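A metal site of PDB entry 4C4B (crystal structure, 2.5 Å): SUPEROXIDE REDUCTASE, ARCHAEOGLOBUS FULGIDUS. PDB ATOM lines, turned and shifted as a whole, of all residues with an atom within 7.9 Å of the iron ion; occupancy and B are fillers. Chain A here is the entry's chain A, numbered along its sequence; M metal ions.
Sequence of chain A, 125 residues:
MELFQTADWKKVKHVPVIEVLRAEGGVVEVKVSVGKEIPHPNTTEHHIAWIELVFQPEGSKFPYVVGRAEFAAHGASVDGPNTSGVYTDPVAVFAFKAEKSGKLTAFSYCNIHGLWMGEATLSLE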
ATOM      1  N   LYS A  10     -18.274   8.027  -5.735  1.00  0.00           N
ATOM      2  CA  LYS A  10     -19.625   8.142  -6.231  1.00  0.00           C
ATOM      3  C   LYS A  10     -20.618   7.441  -5.320  1.00  0.00           C
ATOM      4  O   LYS A  10     -21.798   7.815  -5.259  1.00  0.00           O
ATOM      5  CB  LYS A  10     -19.733   7.574  -7.653  1.00  0.00           C
ATOM      6  CG  LYS A  10     -18.893   8.309  -8.685  1.00  0.00           C
ATOM      7  CD  LYS A  10     -18.967   7.611 -10.037  1.00  0.00           C
ATOM      8  CE  LYS A  10     -18.267   8.422 -11.107  1.00  0.00           C
ATOM      9  NZ  LYS A  10     -18.451   7.822 -12.464  1.00  0.00           N
ATOM     10  N   LYS A  13     -20.948   9.677  -2.312  1.00  0.00           N
ATOM     11  CA  LYS A  13     -21.758  10.818  -2.695  1.00  0.00           C
ATOM     12  C   LYS A  13     -23.249  10.509  -2.620  1.00  0.00           C
ATOM     13  O   LYS A  13     -24.052  11.413  -2.416  1.00  0.00           O
ATOM     14  CB  LYS A  13     -21.356  11.287  -4.108  1.00  0.00           C
ATOM     15  CG  LYS A  13     -22.270  12.309  -4.755  1.00  0.00           C
ATOM     16  CD  LYS A  13     -21.884  12.571  -6.213  1.00  0.00           C
ATOM     17  CE  LYS A  13     -21.638  11.259  -6.967  1.00  0.00           C
ATOM     18  NZ  LYS A  13     -21.610  11.454  -8.461  1.00  0.00           N
ATOM     19  N   HIS A  14     -23.617   9.234  -2.691  1.00  0.00           N
ATOM     20  CA  HIS A  14     -25.039   8.860  -2.752  1.00  0.00           C
ATOM     21  C   HIS A  14     -25.592   8.220  -1.492  1.00  0.00           C
ATOM     22  O   HIS A  14     -26.798   8.230  -1.279  1.00  0.00           O
ATOM     23  CB  HIS A  14     -25.280   7.886  -3.917  1.00  0.00           C
ATOM     24  CG  HIS A  14     -25.405   8.540  -5.261  1.00  0.00           C
ATOM     25  ND1 HIS A  14     -24.367   8.601  -6.163  1.00  0.00           N
ATOM     26  CD2 HIS A  14     -26.468   9.108  -5.873  1.00  0.00           C
ATOM     27  CE1 HIS A  14     -24.768   9.208  -7.266  1.00  0.00           C
ATOM     28  NE2 HIS A  14     -26.045   9.526  -7.115  1.00  0.00           N
ATOM     29  N   VAL A  34     -27.854  12.851   2.451  1.00  0.00           N
ATOM     30  CA  VAL A  34     -27.134  12.350   1.295  1.00  0.00           C
ATOM     31  C   VAL A  34     -26.215  13.453   0.778  1.00  0.00           C
ATOM     32  O   VAL A  34     -26.637  14.603   0.630  1.00  0.00           O
ATOM     33  CB  VAL A  34     -28.108  11.924   0.171  1.00  0.00           C
ATOM     34  CG1 VAL A  34     -27.352  11.536  -1.097  1.00  0.00           C
ATOM     35  CG2 VAL A  34     -29.026  10.791   0.658  1.00  0.00           C
ATOM     36  N   HIS A  40     -23.801  16.078  -3.422  1.00  0.00           N
ATOM     37  CA  HIS A  40     -24.521  15.548  -4.581  1.00  0.00           C
ATOM     38  C   HIS A  40     -25.294  16.707  -5.244  1.00  0.00           C
ATOM     39  O   HIS A  40     -25.898  17.534  -4.557  1.00  0.00           O
ATOM     40  CB  HIS A  40     -25.502  14.450  -4.155  1.00  0.00           C
ATOM     41  CG  HIS A  40     -26.195  13.776  -5.296  1.00  0.00           C
ATOM     42  ND1 HIS A  40     -27.302  14.316  -5.912  1.00  0.00           N
ATOM     43  CD2 HIS A  40     -25.956  12.595  -5.917  1.00  0.00           C
ATOM     44  CE1 HIS A  40     -27.699  13.506  -6.893  1.00  0.00           C
ATOM     45  NE2 HIS A  40     -26.901  12.449  -6.908  1.00  0.00           N
ATOM     46  N   PRO A  41     -25.274  16.760  -6.584  1.00  0.00           N
ATOM     47  CA  PRO A  41     -25.991  17.812  -7.335  1.00  0.00           C
ATOM     48  C   PRO A  41     -27.456  17.951  -6.920  1.00  0.00           C
ATOM     49  O   PRO A  41     -28.086  16.970  -6.502  1.00  0.00           O
ATOM     50  CB  PRO A  41     -25.925  17.308  -8.778  1.00  0.00           C
ATOM     51  CG  PRO A  41     -24.685  16.446  -8.829  1.00  0.00           C
ATOM     52  CD  PRO A  41     -24.600  15.791  -7.475  1.00  0.00           C
ATOM     53  N   HIS A  46     -31.075  16.443 -12.126  1.00  0.00           N
ATOM     54  CA  HIS A  46     -30.376  15.461 -11.295  1.00  0.00           C
ATOM     55  C   HIS A  46     -30.452  15.811  -9.811  1.00  0.00           C
ATOM     56  O   HIS A  46     -29.847  16.779  -9.370  1.00  0.00           O
ATOM     57  CB  HIS A  46     -28.926  15.386 -11.752  1.00  0.00           C
ATOM     58  CG  HIS A  46     -28.104  14.309 -11.076  1.00  0.00           C
ATOM     59  ND1 HIS A  46     -26.729  14.239 -11.224  1.00  0.00           N
ATOM     60  CD2 HIS A  46     -28.460  13.281 -10.294  1.00  0.00           C
ATOM     61  CE1 HIS A  46     -26.276  13.203 -10.545  1.00  0.00           C
ATOM     62  NE2 HIS A  46     -27.301  12.607  -9.966  1.00  0.00           N
ATOM     63  N   HIS A  47     -31.156  15.001  -9.046  1.00  0.00           N
ATOM     64  CA  HIS A  47     -31.346  15.259  -7.622  1.00  0.00           C
ATOM     65  C   HIS A  47     -31.735  13.991  -6.847  1.00  0.00           C
ATOM     66  O   HIS A  47     -32.086  12.969  -7.440  1.00  0.00           O
ATOM     67  CB  HIS A  47     -32.458  16.289  -7.447  1.00  0.00           C
ATOM     68  CG  HIS A  47     -33.644  16.013  -8.298  1.00  0.00           C
ATOM     69  ND1 HIS A  47     -33.819  16.589  -9.546  1.00  0.00           N
ATOM     70  CD2 HIS A  47     -34.682  15.157  -8.134  1.00  0.00           C
ATOM     71  CE1 HIS A  47     -34.924  16.116 -10.097  1.00  0.00           C
ATOM     72  NE2 HIS A  47     -35.459  15.246  -9.267  1.00  0.00           N
ATOM     73  N   ILE A  48     -31.656  14.088  -5.519  1.00  0.00           N
ATOM     74  CA  ILE A  48     -32.127  13.078  -4.591  1.00  0.00           C
ATOM     75  C   ILE A  48     -33.570  13.403  -4.270  1.00  0.00           C
ATOM     76  O   ILE A  48     -33.850  14.538  -3.833  1.00  0.00           O
ATOM     77  CB  ILE A  48     -31.345  13.143  -3.252  1.00  0.00           C
ATOM     78  CG1 ILE A  48     -29.831  13.074  -3.504  1.00  0.00           C
ATOM     79  CG2 ILE A  48     -31.800  12.040  -2.312  1.00  0.00           C
ATOM     80  CD1 ILE A  48     -29.425  11.785  -4.154  1.00  0.00           C
ATOM     81  N   TYR A 109     -33.180   7.765  -2.796  1.00  0.00           N
ATOM     82  CA  TYR A 109     -33.347   7.610  -4.241  1.00  0.00           C
ATOM     83  C   TYR A 109     -32.808   8.810  -4.993  1.00  0.00           C
ATOM     84  O   TYR A 109     -33.146   9.949  -4.684  1.00  0.00           O
ATOM     85  CB  TYR A 109     -34.838   7.382  -4.543  1.00  0.00           C
ATOM     86  CG  TYR A 109     -35.161   7.240  -6.017  1.00  0.00           C
ATOM     87  CD1 TYR A 109     -34.550   6.239  -6.769  1.00  0.00           C
ATOM     88  CD2 TYR A 109     -36.087   8.083  -6.639  1.00  0.00           C
ATOM     89  CE1 TYR A 109     -34.828   6.092  -8.111  1.00  0.00           C
ATOM     90  CE2 TYR A 109     -36.380   7.930  -8.008  1.00  0.00           C
ATOM     91  CZ  TYR A 109     -35.733   6.932  -8.734  1.00  0.00           C
ATOM     92  OH  TYR A 109     -35.972   6.734 -10.078  1.00  0.00           O
ATOM     93  N   CYS A 110     -31.952   8.554  -5.978  1.00  0.00           N
ATOM     94  CA  CYS A 110     -31.530   9.563  -6.951  1.00  0.00           C
ATOM     95  C   CYS A 110     -32.315   9.328  -8.228  1.00  0.00           C
ATOM     96  O   CYS A 110     -32.537   8.175  -8.597  1.00  0.00           O
ATOM     97  CB  CYS A 110     -30.051   9.429  -7.263  1.00  0.00           C
ATOM     98  SG  CYS A 110     -29.393  10.496  -8.563  1.00  0.00           S
ATOM     99  N   ASN A 111     -32.711  10.392  -8.906  1.00  0.00           N
ATOM    100  CA  ASN A 111     -33.572  10.229 -10.075  1.00  0.00           C
ATOM    101  C   ASN A 111     -32.854   9.636 -11.309  1.00  0.00           C
ATOM    102  O   ASN A 111     -33.510   9.268 -12.284  1.00  0.00           O
ATOM    103  CB  ASN A 111     -34.309  11.535 -10.450  1.00  0.00           C
ATOM    104  CG  ASN A 111     -33.416  12.532 -11.134  1.00  0.00           C
ATOM    105  OD1 ASN A 111     -32.237  12.679 -10.777  1.00  0.00           O
ATOM    106  ND2 ASN A 111     -33.961  13.219 -12.129  1.00  0.00           N
ATOM    107  N   ILE A 112     -31.535   9.560 -11.286  1.00  0.00           N
ATOM    108  CA  ILE A 112     -30.826   8.893 -12.382  1.00  0.00           C
ATOM    109  C   ILE A 112     -29.846   7.807 -11.912  1.00  0.00           C
ATOM    110  O   ILE A 112     -29.393   6.999 -12.714  1.00  0.00           O
ATOM    111  CB  ILE A 112     -30.043   9.871 -13.280  1.00  0.00           C
ATOM    112  CG1 ILE A 112     -28.822  10.444 -12.532  1.00  0.00           C
ATOM    113  CG2 ILE A 112     -30.943  10.981 -13.804  1.00  0.00           C
ATOM    114  CD1 ILE A 112     -28.041  11.525 -13.309  1.00  0.00           C
ATOM    115  N   HIS A 113     -29.522   7.771 -10.626  1.00  0.00           N
ATOM    116  CA  HIS A 113     -28.501   6.849 -10.104  1.00  0.00           C
ATOM    117  C   HIS A 113     -29.033   5.741  -9.178  1.00  0.00           C
ATOM    118  O   HIS A 113     -28.274   5.116  -8.455  1.00  0.00           O
ATOM    119  CB  HIS A 113     -27.382   7.632  -9.387  1.00  0.00           C
ATOM    120  CG  HIS A 113     -26.491   8.420 -10.304  1.00  0.00           C
ATOM    121  ND1 HIS A 113     -26.189   9.753 -10.087  1.00  0.00           N
ATOM    122  CD2 HIS A 113     -25.813   8.057 -11.426  1.00  0.00           C
ATOM    123  CE1 HIS A 113     -25.387  10.178 -11.050  1.00  0.00           C
ATOM    124  NE2 HIS A 113     -25.146   9.166 -11.867  1.00  0.00           N
ATOM    125  N   GLY A 114     -30.340   5.506  -9.218  1.00  0.00           N
ATOM    126  CA  GLY A 114     -30.943   4.368  -8.554  1.00  0.00           C
ATOM    127  C   GLY A 114     -31.231   4.487  -7.059  1.00  0.00           C
ATOM    128  O   GLY A 114     -31.345   5.579  -6.510  1.00  0.00           O
ATOM    129  N   TRP A 116     -30.644   3.475  -2.897  1.00  0.00           N
ATOM    130  CA  TRP A 116     -29.487   3.398  -2.007  1.00  0.00           C
ATOM    131  C   TRP A 116     -29.935   3.036  -0.605  1.00  0.00           C
ATOM    132  O   TRP A 116     -31.082   3.273  -0.216  1.00  0.00           O
ATOM    133  CB  TRP A 116     -28.681   4.723  -2.042  1.00  0.00           C
ATOM    134  CG  TRP A 116     -28.083   4.981  -3.403  1.00  0.00           C
ATOM    135  CD1 TRP A 116     -28.734   5.494  -4.498  1.00  0.00           C
ATOM    136  CD2 TRP A 116     -26.740   4.723  -3.832  1.00  0.00           C
ATOM    137  NE1 TRP A 116     -27.876   5.554  -5.572  1.00  0.00           N
ATOM    138  CE2 TRP A 116     -26.650   5.103  -5.197  1.00  0.00           C
ATOM    139  CE3 TRP A 116     -25.601   4.226  -3.197  1.00  0.00           C
ATOM    140  CZ2 TRP A 116     -25.480   4.983  -5.927  1.00  0.00           C
ATOM    141  CZ3 TRP A 116     -24.432   4.098  -3.933  1.00  0.00           C
ATOM    142  CH2 TRP A 116     -24.382   4.484  -5.281  1.00  0.00           C
HETATM  143 FE    FE M   1     -27.033  10.957  -8.496  1.00  0.00          FE
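O of Lys 10 sits at hydrogen-bond distance from ND1 of His 14, at 2.8 Å.
SG of Cys 110 lies close to N of Ile 112 (3.6 Å).
The indole nitrogen (NE1) of Trp 116 is in hydrogen-bond range of the backbone carbonyl oxygen (O) of His 113 (2.9 Å).
Of the 16 residues printed, 5 come within 4 Å of the iron ion.
The nearest printed residue that does not touch the iron ion is Ile 112 (4.4 Å).
The iron ion is bound by ND1 of His 113 (2.2 Å), NE2 of His 40 (2.2 Å), NE2 of His 14 (2.2 Å), NE2 of His 46 (2.2 Å) and SG of Cys 110 (2.4 Å).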
